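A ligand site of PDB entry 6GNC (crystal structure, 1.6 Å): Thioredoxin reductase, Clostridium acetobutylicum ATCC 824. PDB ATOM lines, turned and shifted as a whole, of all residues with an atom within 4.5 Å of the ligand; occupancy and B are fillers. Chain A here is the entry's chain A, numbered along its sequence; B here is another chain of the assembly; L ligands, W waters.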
ATOM      1  N   ILE A  12     -23.638  19.217  10.105  1.00  0.00           N
ATOM      2  CA  ILE A  12     -24.216  18.749  11.358  1.00  0.00           C
ATOM      3  C   ILE A  12     -23.140  18.820  12.433  1.00  0.00           C
ATOM      4  O   ILE A  12     -22.325  17.908  12.571  1.00  0.00           O
ATOM      5  CB  ILE A  12     -24.784  17.334  11.247  1.00  0.00           C
ATOM      6  CG1 ILE A  12     -25.761  17.336  10.065  1.00  0.00           C
ATOM      7  CG2 ILE A  12     -25.491  16.942  12.552  1.00  0.00           C
ATOM      8  CD1 ILE A  12     -26.194  15.991   9.663  1.00  0.00           C
ATOM      9  N   GLY A  13     -23.207  19.875  13.219  1.00  0.00           N
ATOM     10  CA  GLY A  13     -22.284  20.092  14.315  1.00  0.00           C
ATOM     11  C   GLY A  13     -21.639  21.469  14.271  1.00  0.00           C
ATOM     12  O   GLY A  13     -21.272  21.960  13.204  1.00  0.00           O
ATOM     13  N   SER A  14     -21.454  22.043  15.462  1.00  0.00           N
ATOM     14  CA  SER A  14     -21.012  23.417  15.640  1.00  0.00           C
ATOM     15  C   SER A  14     -19.762  23.540  16.507  1.00  0.00           C
ATOM     16  O   SER A  14     -19.490  24.599  17.070  1.00  0.00           O
ATOM     17  CB  SER A  14     -22.148  24.262  16.231  1.00  0.00           C
ATOM     18  OG  SER A  14     -22.605  23.742  17.475  1.00  0.00           O
ATOM     19  N   GLY A  15     -19.024  22.458  16.656  1.00  0.00           N
ATOM     20  CA  GLY A  15     -17.676  22.535  17.199  1.00  0.00           C
ATOM     21  C   GLY A  15     -16.710  23.034  16.153  1.00  0.00           C
ATOM     22  O   GLY A  15     -17.087  23.424  15.056  1.00  0.00           O
ATOM     23  N   PRO A  16     -15.408  23.003  16.458  1.00  0.00           N
ATOM     24  CA  PRO A  16     -14.453  23.559  15.481  1.00  0.00           C
ATOM     25  C   PRO A  16     -14.501  22.898  14.120  1.00  0.00           C
ATOM     26  O   PRO A  16     -14.251  23.590  13.122  1.00  0.00           O
ATOM     27  CB  PRO A  16     -13.089  23.333  16.174  1.00  0.00           C
ATOM     28  CG  PRO A  16     -13.339  22.258  17.186  1.00  0.00           C
ATOM     29  CD  PRO A  16     -14.743  22.546  17.695  1.00  0.00           C
ATOM     30  N   ALA A  17     -14.779  21.594  14.027  1.00  0.00           N
ATOM     31  CA  ALA A  17     -14.886  20.969  12.709  1.00  0.00           C
ATOM     32  C   ALA A  17     -16.023  21.602  11.901  1.00  0.00           C
ATOM     33  O   ALA A  17     -15.813  22.028  10.765  1.00  0.00           O
ATOM     34  CB  ALA A  17     -15.101  19.459  12.838  1.00  0.00           C
ATOM     35  N   GLY A  18     -17.219  21.693  12.474  1.00  0.00           N
ATOM     36  CA  GLY A  18     -18.343  22.249  11.737  1.00  0.00           C
ATOM     37  C   GLY A  18     -18.173  23.713  11.399  1.00  0.00           C
ATOM     38  O   GLY A  18     -18.532  24.176  10.309  1.00  0.00           O
ATOM     39  N   PHE A  35     -26.022  23.381  11.625  1.00  0.00           N
ATOM     40  CA  PHE A  35     -26.824  22.960  12.760  1.00  0.00           C
ATOM     41  C   PHE A  35     -25.954  22.783  13.986  1.00  0.00           C
ATOM     42  O   PHE A  35     -24.831  22.258  13.887  1.00  0.00           O
ATOM     43  CB  PHE A  35     -27.558  21.660  12.501  1.00  0.00           C
ATOM     44  CG  PHE A  35     -28.524  21.692  11.372  1.00  0.00           C
ATOM     45  CD1 PHE A  35     -29.807  22.139  11.568  1.00  0.00           C
ATOM     46  CD2 PHE A  35     -28.168  21.223  10.113  1.00  0.00           C
ATOM     47  CE1 PHE A  35     -30.705  22.150  10.530  1.00  0.00           C
ATOM     48  CE2 PHE A  35     -29.069  21.230   9.084  1.00  0.00           C
ATOM     49  CZ  PHE A  35     -30.342  21.694   9.291  1.00  0.00           C
ATOM     50  N   GLY A  36     -26.481  23.152  15.132  1.00  0.00           N
ATOM     51  CA  GLY A  36     -25.758  22.912  16.374  1.00  0.00           C
ATOM     52  C   GLY A  36     -26.247  23.754  17.525  1.00  0.00           C
ATOM     53  O   GLY A  36     -27.452  23.970  17.671  1.00  0.00           O
ATOM     54  N   SER A  37     -25.305  24.255  18.323  1.00  0.00           N
ATOM     55  CA  SER A  37     -25.581  24.934  19.579  1.00  0.00           C
ATOM     56  C   SER A  37     -24.997  26.342  19.542  1.00  0.00           C
ATOM     57  O   SER A  37     -23.908  26.554  19.009  1.00  0.00           O
ATOM     58  CB  SER A  37     -24.994  24.126  20.741  1.00  0.00           C
ATOM     59  OG  SER A  37     -25.038  24.843  21.962  1.00  0.00           O
ATOM     60  N   LEU A  40     -21.757  26.477  20.849  1.00  0.00           N
ATOM     61  CA  LEU A  40     -20.819  25.791  19.971  1.00  0.00           C
ATOM     62  C   LEU A  40     -20.583  24.329  20.391  1.00  0.00           C
ATOM     63  O   LEU A  40     -20.930  23.395  19.657  1.00  0.00           O
ATOM     64  CB  LEU A  40     -19.478  26.537  19.941  1.00  0.00           C
ATOM     65  CG  LEU A  40     -19.499  27.938  19.342  1.00  0.00           C
ATOM     66  CD1 LEU A  40     -18.146  28.612  19.512  1.00  0.00           C
ATOM     67  CD2 LEU A  40     -19.899  27.895  17.873  1.00  0.00           C
ATOM     68  N   SER A  41     -19.969  24.130  21.550  1.00  0.00           N
ATOM     69  CA  SER A  41     -19.603  22.801  22.016  1.00  0.00           C
ATOM     70  C   SER A  41     -19.442  22.839  23.522  1.00  0.00           C
ATOM     71  O   SER A  41     -18.777  23.726  24.047  1.00  0.00           O
ATOM     72  CB  SER A  41     -18.291  22.334  21.371  1.00  0.00           C
ATOM     73  OG  SER A  41     -17.809  21.161  21.994  1.00  0.00           O
ATOM     74  N   LYS A  43     -17.643  20.907  25.077  1.00  0.00           N
ATOM     75  CA  LYS A  43     -16.258  20.517  25.366  1.00  0.00           C
ATOM     76  C   LYS A  43     -15.323  21.699  25.310  1.00  0.00           C
ATOM     77  O   LYS A  43     -14.316  21.731  26.023  1.00  0.00           O
ATOM     78  CB  LYS A  43     -15.794  19.446  24.398  1.00  0.00           C
ATOM     79  CG  LYS A  43     -16.512  18.146  24.605  1.00  0.00           C
ATOM     80  CD  LYS A  43     -15.944  17.021  23.772  1.00  0.00           C
ATOM     81  CE  LYS A  43     -16.683  15.740  24.153  1.00  0.00           C
ATOM     82  NZ  LYS A  43     -16.259  14.575  23.335  1.00  0.00           N
ATOM     83  N   LYS A  46     -15.887  23.602  28.708  1.00  0.00           N
ATOM     84  CA  LYS A  46     -15.184  22.932  29.810  1.00  0.00           C
ATOM     85  C   LYS A  46     -13.672  23.166  29.996  1.00  0.00           C
ATOM     86  O   LYS A  46     -13.183  23.217  31.118  1.00  0.00           O
ATOM     87  CB  LYS A  46     -15.479  21.436  29.771  1.00  0.00           C
ATOM     88  CG  LYS A  46     -16.913  21.101  30.125  1.00  0.00           C
ATOM     89  CD  LYS A  46     -17.126  19.596  30.246  1.00  0.00           C
ATOM     90  CE  LYS A  46     -18.522  19.288  30.752  1.00  0.00           C
ATOM     91  NZ  LYS A  46     -19.575  19.884  29.883  1.00  0.00           N
ATOM     92  N   ALA A  47     -12.919  23.291  28.902  1.00  0.00           N
ATOM     93  CA  ALA A  47     -11.454  23.391  28.998  1.00  0.00           C
ATOM     94  C   ALA A  47     -10.907  24.623  29.752  1.00  0.00           C
ATOM     95  O   ALA A  47     -11.301  25.750  29.457  1.00  0.00           O
ATOM     96  CB  ALA A  47     -10.860  23.364  27.598  1.00  0.00           C
ATOM     97  N   LYS A  49      -7.419  25.893  30.131  1.00  0.00           N
ATOM     98  CA  LYS A  49      -6.376  26.655  29.440  1.00  0.00           C
ATOM     99  C   LYS A  49      -6.022  25.871  28.194  1.00  0.00           C
ATOM    100  O   LYS A  49      -5.899  24.660  28.248  1.00  0.00           O
ATOM    101  CB  LYS A  49      -5.142  26.839  30.320  1.00  0.00           C
ATOM    102  CG  LYS A  49      -5.254  27.969  31.323  1.00  0.00           C
ATOM    103  CD  LYS A  49      -5.310  29.316  30.629  1.00  0.00           C
ATOM    104  CE  LYS A  49      -5.242  30.459  31.626  1.00  0.00           C
ATOM    105  NZ  LYS A  49      -5.224  31.783  30.956  1.00  0.00           N
ATOM    106  N   ILE A  50      -5.795  26.552  27.080  1.00  0.00           N
ATOM    107  CA  ILE A  50      -5.547  25.835  25.832  1.00  0.00           C
ATOM    108  C   ILE A  50      -4.315  26.452  25.190  1.00  0.00           C
ATOM    109  O   ILE A  50      -4.336  27.643  24.848  1.00  0.00           O
ATOM    110  CB  ILE A  50      -6.749  25.899  24.873  1.00  0.00           C
ATOM    111  CG1 ILE A  50      -8.002  25.326  25.540  1.00  0.00           C
ATOM    112  CG2 ILE A  50      -6.392  25.254  23.520  1.00  0.00           C
ATOM    113  CD1 ILE A  50      -9.329  25.855  24.933  1.00  0.00           C
ATOM    114  N   ASN A  52      -2.488  24.514  22.692  1.00  0.00           N
ATOM    115  CA  ASN A  52      -2.210  23.762  21.471  1.00  0.00           C
ATOM    116  C   ASN A  52      -2.984  24.165  20.186  1.00  0.00           C
ATOM    117  O   ASN A  52      -3.010  23.382  19.246  1.00  0.00           O
ATOM    118  CB  ASN A  52      -2.351  22.262  21.720  1.00  0.00           C
ATOM    119  CG  ASN A  52      -3.781  21.849  21.982  1.00  0.00           C
ATOM    120  OD1 ASN A  52      -4.649  22.675  22.211  1.00  0.00           O
ATOM    121  ND2 ASN A  52      -4.038  20.547  21.930  1.00  0.00           N
ATOM    122  N   GLU A  82     -31.124  23.696  16.151  1.00  0.00           N
ATOM    123  CA  GLU A  82     -32.043  22.592  16.064  1.00  0.00           C
ATOM    124  C   GLU A  82     -31.222  21.322  16.001  1.00  0.00           C
ATOM    125  O   GLU A  82     -30.118  21.324  15.466  1.00  0.00           O
ATOM    126  CB  GLU A  82     -32.936  22.740  14.829  1.00  0.00           C
ATOM    127  CG  GLU A  82     -33.848  23.954  14.894  1.00  0.00           C
ATOM    128  CD  GLU A  82     -34.493  24.300  13.565  1.00  0.00           C
ATOM    129  OE1 GLU A  82     -33.955  23.886  12.517  1.00  0.00           O
ATOM    130  OE2 GLU A  82     -35.528  24.984  13.561  1.00  0.00           O
ATOM    131  N   LYS A  83     -31.756  20.235  16.528  1.00  0.00           N
ATOM    132  CA  LYS A  83     -31.027  18.982  16.547  1.00  0.00           C
ATOM    133  C   LYS A  83     -31.460  18.106  15.365  1.00  0.00           C
ATOM    134  O   LYS A  83     -32.640  17.843  15.212  1.00  0.00           O
ATOM    135  CB  LYS A  83     -31.301  18.250  17.863  1.00  0.00           C
ATOM    136  CG  LYS A  83     -30.838  16.806  17.892  1.00  0.00           C
ATOM    137  CD  LYS A  83     -31.009  16.215  19.284  1.00  0.00           C
ATOM    138  CE  LYS A  83     -30.656  14.735  19.319  1.00  0.00           C
ATOM    139  NZ  LYS A  83     -31.675  13.902  18.616  1.00  0.00           N
ATOM    140  N   VAL A  84     -30.514  17.663  14.535  1.00  0.00           N
ATOM    141  CA  VAL A  84     -30.847  16.811  13.419  1.00  0.00           C
ATOM    142  C   VAL A  84     -31.033  15.409  13.975  1.00  0.00           C
ATOM    143  O   VAL A  84     -30.180  14.906  14.698  1.00  0.00           O
ATOM    144  CB  VAL A  84     -29.742  16.810  12.353  1.00  0.00           C
ATOM    145  CG1 VAL A  84     -30.117  15.886  11.201  1.00  0.00           C
ATOM    146  CG2 VAL A  84     -29.496  18.218  11.853  1.00  0.00           C
ATOM    147  N   ALA A 111     -20.162  16.395  11.576  1.00  0.00           N
ATOM    148  CA  ALA A 111     -19.153  17.032  12.460  1.00  0.00           C
ATOM    149  C   ALA A 111     -19.695  17.044  13.892  1.00  0.00           C
ATOM    150  O   ALA A 111     -19.627  18.031  14.609  1.00  0.00           O
ATOM    151  CB  ALA A 111     -18.848  18.423  11.924  1.00  0.00           C
ATOM    152  N   SER A 112     -20.203  15.890  14.326  1.00  0.00           N
ATOM    153  CA  SER A 112     -21.036  15.802  15.505  1.00  0.00           C
ATOM    154  C   SER A 112     -20.291  15.507  16.796  1.00  0.00           C
ATOM    155  O   SER A 112     -20.908  15.485  17.856  1.00  0.00           O
ATOM    156  CB  SER A 112     -22.116  14.719  15.285  1.00  0.00           C
ATOM    157  OG  SER A 112     -21.509  13.483  14.894  1.00  0.00           O
ATOM    158  N   GLY A 113     -18.975  15.322  16.723  1.00  0.00           N
ATOM    159  CA  GLY A 113     -18.207  14.937  17.877  1.00  0.00           C
ATOM    160  C   GLY A 113     -18.435  13.490  18.249  1.00  0.00           C
ATOM    161  O   GLY A 113     -18.988  12.673  17.482  1.00  0.00           O
ATOM    162  N   ASP A 222     -25.147  15.188  23.988  1.00  0.00           N
ATOM    163  CA  ASP A 222     -24.748  16.190  23.011  1.00  0.00           C
ATOM    164  C   ASP A 222     -24.747  15.676  21.573  1.00  0.00           C
ATOM    165  O   ASP A 222     -24.676  16.490  20.646  1.00  0.00           O
ATOM    166  CB  ASP A 222     -23.354  16.724  23.358  1.00  0.00           C
ATOM    167  CG  ASP A 222     -23.364  17.653  24.552  1.00  0.00           C
ATOM    168  OD1 ASP A 222     -24.328  18.437  24.686  1.00  0.00           O
ATOM    169  OD2 ASP A 222     -22.412  17.598  25.356  1.00  0.00           O
ATOM    170  N   SER A 223     -24.799  14.369  21.366  1.00  0.00           N
ATOM    171  CA  SER A 223     -24.813  13.826  20.013  1.00  0.00           C
ATOM    172  C   SER A 223     -25.295  12.373  20.073  1.00  0.00           C
ATOM    173  O   SER A 223     -25.344  11.768  21.141  1.00  0.00           O
ATOM    174  CB  SER A 223     -23.436  13.878  19.369  1.00  0.00           C
ATOM    175  OG  SER A 223     -22.632  12.857  19.947  1.00  0.00           O
ATOM    176  N   LEU A 229     -27.484   8.220  13.100  1.00  0.00           N
ATOM    177  CA  LEU A 229     -27.910   9.467  12.461  1.00  0.00           C
ATOM    178  C   LEU A 229     -28.059   9.292  10.963  1.00  0.00           C
ATOM    179  O   LEU A 229     -29.024   9.805  10.359  1.00  0.00           O
ATOM    180  CB  LEU A 229     -26.868  10.560  12.754  1.00  0.00           C
ATOM    181  CG  LEU A 229     -27.012  11.973  12.155  1.00  0.00           C
ATOM    182  CD1 LEU A 229     -28.242  12.587  12.838  1.00  0.00           C
ATOM    183  CD2 LEU A 229     -25.789  12.848  12.322  1.00  0.00           C
ATOM    184  N   ALA A 256     -15.832  15.020   9.698  1.00  0.00           N
ATOM    185  CA  ALA A 256     -14.699  15.793  10.248  1.00  0.00           C
ATOM    186  C   ALA A 256     -14.761  15.878  11.752  1.00  0.00           C
ATOM    187  O   ALA A 256     -15.842  15.954  12.354  1.00  0.00           O
ATOM    188  CB  ALA A 256     -14.730  17.204   9.650  1.00  0.00           C
ATOM    189  N   GLY A 257     -13.568  15.944  12.367  1.00  0.00           N
ATOM    190  CA  GLY A 257     -13.466  16.133  13.811  1.00  0.00           C
ATOM    191  C   GLY A 257     -13.411  14.832  14.572  1.00  0.00           C
ATOM    192  O   GLY A 257     -13.039  13.771  14.051  1.00  0.00           O
ATOM    193  N   ASP A 258     -13.802  14.904  15.851  1.00  0.00           N
ATOM    194  CA  ASP A 258     -13.706  13.739  16.723  1.00  0.00           C
ATOM    195  C   ASP A 258     -14.482  12.568  16.121  1.00  0.00           C
ATOM    196  O   ASP A 258     -14.090  11.404  16.283  1.00  0.00           O
ATOM    197  CB  ASP A 258     -14.259  14.026  18.132  1.00  0.00           C
ATOM    198  CG  ASP A 258     -13.399  14.935  19.005  1.00  0.00           C
ATOM    199  OD1 ASP A 258     -12.266  15.350  18.604  1.00  0.00           O
ATOM    200  OD2 ASP A 258     -13.867  15.201  20.155  1.00  0.00           O
ATOM    201  N   TYR A 264      -8.366  13.462  19.615  1.00  0.00           N
ATOM    202  CA  TYR A 264      -9.456  14.403  19.794  1.00  0.00           C
ATOM    203  C   TYR A 264      -8.831  15.736  20.171  1.00  0.00           C
ATOM    204  O   TYR A 264      -8.454  15.951  21.323  1.00  0.00           O
ATOM    205  CB  TYR A 264     -10.401  13.932  20.894  1.00  0.00           C
ATOM    206  CG  TYR A 264     -11.062  12.591  20.651  1.00  0.00           C
ATOM    207  CD1 TYR A 264     -11.461  12.211  19.380  1.00  0.00           C
ATOM    208  CD2 TYR A 264     -11.305  11.723  21.695  1.00  0.00           C
ATOM    209  CE1 TYR A 264     -12.069  10.994  19.155  1.00  0.00           C
ATOM    210  CE2 TYR A 264     -11.924  10.503  21.475  1.00  0.00           C
ATOM    211  CZ  TYR A 264     -12.302  10.142  20.209  1.00  0.00           C
ATOM    212  OH  TYR A 264     -12.912   8.930  19.997  1.00  0.00           O
ATOM    213  N   GLN A 265      -8.741  16.624  19.204  1.00  0.00           N
ATOM    214  CA  GLN A 265      -8.171  17.950  19.388  1.00  0.00           C
ATOM    215  C   GLN A 265      -8.845  19.006  18.523  1.00  0.00           C
ATOM    216  O   GLN A 265      -9.389  18.700  17.448  1.00  0.00           O
ATOM    217  CB  GLN A 265      -6.664  17.955  19.028  1.00  0.00           C
ATOM    218  CG  GLN A 265      -5.822  16.881  19.673  1.00  0.00           C
ATOM    219  CD  GLN A 265      -5.223  17.335  20.973  1.00  0.00           C
ATOM    220  OE1 GLN A 265      -4.031  17.718  21.059  1.00  0.00           O
ATOM    221  NE2 GLN A 265      -6.034  17.302  22.012  1.00  0.00           N
ATOM    222  N   TYR A 266      -8.769  20.261  18.978  1.00  0.00           N
ATOM    223  CA  TYR A 266      -9.501  21.344  18.314  1.00  0.00           C
ATOM    224  C   TYR A 266      -8.971  21.609  16.905  1.00  0.00           C
ATOM    225  O   TYR A 266      -9.741  21.744  15.954  1.00  0.00           O
ATOM    226  CB  TYR A 266      -9.432  22.661  19.106  1.00  0.00           C
ATOM    227  CG  TYR A 266      -9.971  22.659  20.521  1.00  0.00           C
ATOM    228  CD1 TYR A 266     -11.314  22.374  20.791  1.00  0.00           C
ATOM    229  CD2 TYR A 266      -9.149  22.983  21.578  1.00  0.00           C
ATOM    230  CE1 TYR A 266     -11.794  22.377  22.100  1.00  0.00           C
ATOM    231  CE2 TYR A 266      -9.617  22.980  22.877  1.00  0.00           C
ATOM    232  CZ  TYR A 266     -10.938  22.688  23.138  1.00  0.00           C
ATOM    233  OH  TYR A 266     -11.375  22.703  24.445  1.00  0.00           O
ATOM    234  N   SER A 269      -9.553  19.062  14.370  1.00  0.00           N
ATOM    235  CA  SER A 269     -10.963  19.089  13.960  1.00  0.00           C
ATOM    236  C   SER A 269     -11.219  20.189  12.949  1.00  0.00           C
ATOM    237  O   SER A 269     -11.923  19.994  11.945  1.00  0.00           O
ATOM    238  CB  SER A 269     -11.887  19.252  15.171  1.00  0.00           C
ATOM    239  OG  SER A 269     -11.770  18.147  16.032  1.00  0.00           O
ATOM    240  N   GLN B 274      -0.542  18.584  13.993  1.00  0.00           N
ATOM    241  CA  GLN B 274      -0.908  18.071  15.291  1.00  0.00           C
ATOM    242  C   GLN B 274      -1.083  16.560  15.260  1.00  0.00           C
ATOM    243  O   GLN B 274      -0.602  15.863  16.164  1.00  0.00           O
ATOM    244  CB  GLN B 274      -2.168  18.823  15.753  1.00  0.00           C
ATOM    245  CG  GLN B 274      -2.757  18.294  17.019  1.00  0.00           C
ATOM    246  CD  GLN B 274      -3.922  19.106  17.424  1.00  0.00           C
ATOM    247  OE1 GLN B 274      -4.960  19.078  16.750  1.00  0.00           O
ATOM    248  NE2 GLN B 274      -3.789  19.876  18.508  1.00  0.00           N
HETATM  249  P1  LIG L   1     -17.516  18.915  19.280  1.00  0.00           P
HETATM  250  O1  LIG L   1     -16.578  19.920  19.855  1.00  0.00           O
HETATM  251  O2  LIG L   1     -18.001  17.779  20.121  1.00  0.00           O
HETATM  252  O3  LIG L   1     -18.770  19.723  18.690  1.00  0.00           O
HETATM  253  C1  LIG L   1     -19.929  19.036  18.241  1.00  0.00           C
HETATM  254  C2  LIG L   1     -21.150  19.939  18.384  1.00  0.00           C
HETATM  255  O4  LIG L   1     -22.159  19.545  17.454  1.00  0.00           O
HETATM  256  C3  LIG L   1     -21.740  19.807  19.768  1.00  0.00           C
HETATM  257  O5  LIG L   1     -22.222  21.072  20.212  1.00  0.00           O
HETATM  258  C4  LIG L   1     -22.910  18.880  19.571  1.00  0.00           C
HETATM  259  O6  LIG L   1     -23.929  19.063  20.554  1.00  0.00           O
HETATM  260  C5  LIG L   1     -23.359  19.245  18.175  1.00  0.00           C
HETATM  261  N1  LIG L   1     -24.126  18.141  17.573  1.00  0.00           N
HETATM  262  C6  LIG L   1     -23.811  16.842  17.601  1.00  0.00           C
HETATM  263  N2  LIG L   1     -24.756  16.117  16.949  1.00  0.00           N
HETATM  264  C7  LIG L   1     -25.690  16.961  16.511  1.00  0.00           C
HETATM  265  C8  LIG L   1     -26.958  16.859  15.763  1.00  0.00           C
HETATM  266  N3  LIG L   1     -27.419  15.667  15.343  1.00  0.00           N
HETATM  267  N4  LIG L   1     -27.632  18.000  15.513  1.00  0.00           N
HETATM  268  C9  LIG L   1     -27.190  19.194  15.928  1.00  0.00           C
HETATM  269  N5  LIG L   1     -26.053  19.363  16.608  1.00  0.00           N
HETATM  270  C10 LIG L   1     -25.282  18.300  16.926  1.00  0.00           C
HETATM  271  N6  LIG L   1      -8.522  19.688  22.523  1.00  0.00           N
HETATM  272  C11 LIG L   1      -7.428  20.447  22.283  1.00  0.00           C
HETATM  273  O7  LIG L   1      -6.964  20.461  21.126  1.00  0.00           O
HETATM  274  N7  LIG L   1      -6.823  21.195  23.218  1.00  0.00           N
HETATM  275  C12 LIG L   1      -7.265  21.233  24.476  1.00  0.00           C
HETATM  276  O8  LIG L   1      -6.697  21.932  25.330  1.00  0.00           O
HETATM  277  C13 LIG L   1      -8.458  20.420  24.831  1.00  0.00           C
HETATM  278  N8  LIG L   1      -8.966  20.408  26.079  1.00  0.00           N
HETATM  279  C14 LIG L   1     -10.052  19.666  26.375  1.00  0.00           C
HETATM  280  C15 LIG L   1     -10.558  19.677  27.669  1.00  0.00           C
HETATM  281  C16 LIG L   1     -11.672  18.917  27.982  1.00  0.00           C
HETATM  282  C17 LIG L   1     -12.218  18.919  29.386  1.00  0.00           C
HETATM  283  C18 LIG L   1     -12.331  18.098  26.939  1.00  0.00           C
HETATM  284  C19 LIG L   1     -13.546  17.274  27.293  1.00  0.00           C
HETATM  285  C20 LIG L   1     -11.834  18.089  25.643  1.00  0.00           C
HETATM  286  C21 LIG L   1     -10.721  18.840  25.326  1.00  0.00           C
HETATM  287  N9  LIG L   1     -10.199  18.837  24.017  1.00  0.00           N
HETATM  288  C22 LIG L   1      -9.082  19.633  23.745  1.00  0.00           C
HETATM  289  C23 LIG L   1     -10.831  18.046  22.962  1.00  0.00           C
HETATM  290  C24 LIG L   1     -11.647  18.939  22.044  1.00  0.00           C
HETATM  291  O9  LIG L   1     -12.671  19.573  22.824  1.00  0.00           O
HETATM  292  C25 LIG L   1     -12.294  18.146  20.925  1.00  0.00           C
HETATM  293  O10 LIG L   1     -11.301  17.413  20.215  1.00  0.00           O
HETATM  294  C26 LIG L   1     -13.024  19.059  19.964  1.00  0.00           C
HETATM  295  O11 LIG L   1     -14.001  19.826  20.672  1.00  0.00           O
HETATM  296  C27 LIG L   1     -13.705  18.270  18.859  1.00  0.00           C
HETATM  297  O12 LIG L   1     -14.596  19.157  18.190  1.00  0.00           O
HETATM  298  P2  LIG L   1     -15.636  18.667  17.090  1.00  0.00           P
HETATM  299  O13 LIG L   1     -15.972  19.841  16.227  1.00  0.00           O
HETATM  300  O14 LIG L   1     -15.177  17.395  16.452  1.00  0.00           O
HETATM  301  O15 LIG L   1     -16.920  18.234  17.952  1.00  0.00           O
HETATM  302  O   HOH W   1      -7.431  17.226  25.605  1.00  0.00           O
HETATM  303  O   HOH W   2      -8.822  15.352  23.926  1.00  0.00           O
HETATM  304  O   HOH W   3      -3.871  22.680  25.392  1.00  0.00           O
HETATM  305  O   HOH W   4     -21.368  19.816  23.156  1.00  0.00           O
HETATM  306  O   HOH W   5     -16.580  15.457  20.683  1.00  0.00           O
HETATM  307  O   HOH W   6     -20.650  15.617  20.610  1.00  0.00           O
HETATM  308  O   HOH W   7     -23.617  21.263  22.586  1.00  0.00           O
HETATM  309  O   HOH W   8      -5.806  22.030  19.173  1.00  0.00           O
HETATM  310  O   HOH W   9      -7.543  22.329  28.101  1.00  0.00           O
HETATM  311  O   HOH W  10     -19.681  17.553  22.140  1.00  0.00           O
HETATM  312  O   HOH W  11     -16.728  15.702  15.002  1.00  0.00           O
HETATM  313  O   HOH W  12     -18.232  20.319  14.852  1.00  0.00           O
HETATM  314  O   HOH W  13     -25.490  13.548  16.380  1.00  0.00           O
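An oxygen (O6) of the ligand lies within hydrogen-bond range of the backbone carbonyl oxygen of Asp 222 (2.7 Å). O5 of the ligand is in hydrogen-bond range of O of Leu 40, at 2.7 Å. The side-chain hydroxyl (OG) of Ser 41 sits at hydrogen-bond distance from an oxygen (O1) of the ligand (2.8 Å). O14 of the ligand is in hydrogen-bond range of N of Asp 258 (2.9 Å). O10 of the ligand sits at hydrogen-bond distance from OD1 of Asp 258 (2.8 Å). O7 of the ligand is in hydrogen-bond range of N of Tyr 266, 2.8 Å away. The side-chain amide oxygen (OD1) of Asn 52 lies within hydrogen-bond range of a nitrogen (N7) of the ligand. N of Gln 265 is in hydrogen-bond range of O10 of the ligand (2.9 Å). NE2 of Gln 265 lies close to O7 of the ligand, at 3.4 Å. A nitrogen (N4) of the ligand sits at hydrogen-bond distance from the backbone NH (N) of Val 84, at 3.1 Å. The backbone carbonyl oxygen (O) of Val 84 sits at hydrogen-bond distance from a nitrogen (N3) of the ligand. O of Tyr 264 lies close to O10 of the ligand (3.4 Å). N of Ala 17 is in hydrogen-bond range of O13 of the ligand (3.1 Å). N of Ser 14 sits at hydrogen-bond distance from O4 of the ligand, at 3.3 Å. N of Gly 15 sits close to O3 of the ligand (3.4 Å).
OG of Ser 14 sits at hydrogen-bond distance from O of Leu 40, 2.8 Å away. OG of Ser 41 lies close to N of Lys 43, 3.1 Å away. The side-chain hydroxyl (OH) of Tyr 266 is in hydrogen-bond range of the backbone carbonyl oxygen (O) of Lys 43 (3.5 Å). The side-chain hydroxyl (OG) of Ser 269 lies within hydrogen-bond range of the backbone carbonyl oxygen (O) of Gln 265 (2.8 Å). The side-chain amide oxygen of Gln 265 is in hydrogen-bond range of the side-chain amide nitrogen of Gln 274 of chain B. The backbone NH of Ser 112 sits at hydrogen-bond distance from the backbone carbonyl oxygen of Ile 12, at 3.4 Å. N of Ser 37 lies within hydrogen-bond range of OG of Ser 14. The backbone carbonyl oxygen (O) of Ile 12 sits at hydrogen-bond distance from the backbone NH (N) of Ala 111 (2.8 Å).
The backbone nitrogen of Pro 16 sits close to an oxygen (O13) of the ligand (3.2 Å). Merely in contact with the ligand: Ile 12 (3.5 Å), Gly 13 (3.2 Å), Gly 36 (3.6 Å), Lys 43 (3.5 Å), Ala 47 (3.7 Å), Ile 50 (3.6 Å), Glu 82 (3.7 Å), Lys 83 (3.7 Å), Ala 111 (3.8 Å), Ser 112 (3.2 Å), Gly 113 (3.5 Å), Ser 223 (3.5 Å), Gly 257 (3.4 Å) and Ser 269 (3.4 Å). Hydrophobic or aromatic side chains that line the ligand: Ile 12, Pro 16, Ala 17, Ala 47, Ile 50, Val 84, Tyr 264 and Tyr 266. 27 residues have an atom within 4 Å of the ligand: Ile 12, Gly 13, Ser 14, Gly 15, Pro 16, Ala 17, Gly 36, Leu 40, Ser 41, Lys 43, Ala 47, Ile 50, Asn 52, Glu 82, Lys 83, Val 84, Ala 111, Ser 112, Gly 113, Asp 222, Ser 223, Gly 257, Asp 258, Tyr 264, Gln 265, Tyr 266 and Ser 269.
Water W11 lies within hydrogen-bond range of O14 of the ligand, O of Ala 256, N of Gly 113 and N of Asp 258. Water W8 lies within hydrogen-bond range of an oxygen (O7) of the ligand, the side-chain amide nitrogen (NE2) of Gln 274 of chain B, the backbone carbonyl oxygen (O) of Asn 52 and the backbone NH (N) of Tyr 266. Water W3 lies within hydrogen-bond range of O8 of the ligand (2.9 Å) and OD1 of Asn 52 (3.3 Å). Water W9 bridges the backbone carbonyl oxygen (O) of Lys 49 and an oxygen (O8) of the ligand. Water W4 lies within hydrogen-bond range of OD2 of Asp 222 (3.3 Å) and O5 of the ligand (3.3 Å). Water W6 lies within hydrogen-bond range of the backbone carbonyl oxygen of Ser 112 (2.8 Å), an oxygen (O2) of the ligand (3.5 Å) and the side-chain hydroxyl of Ser 223 (3.5 Å).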
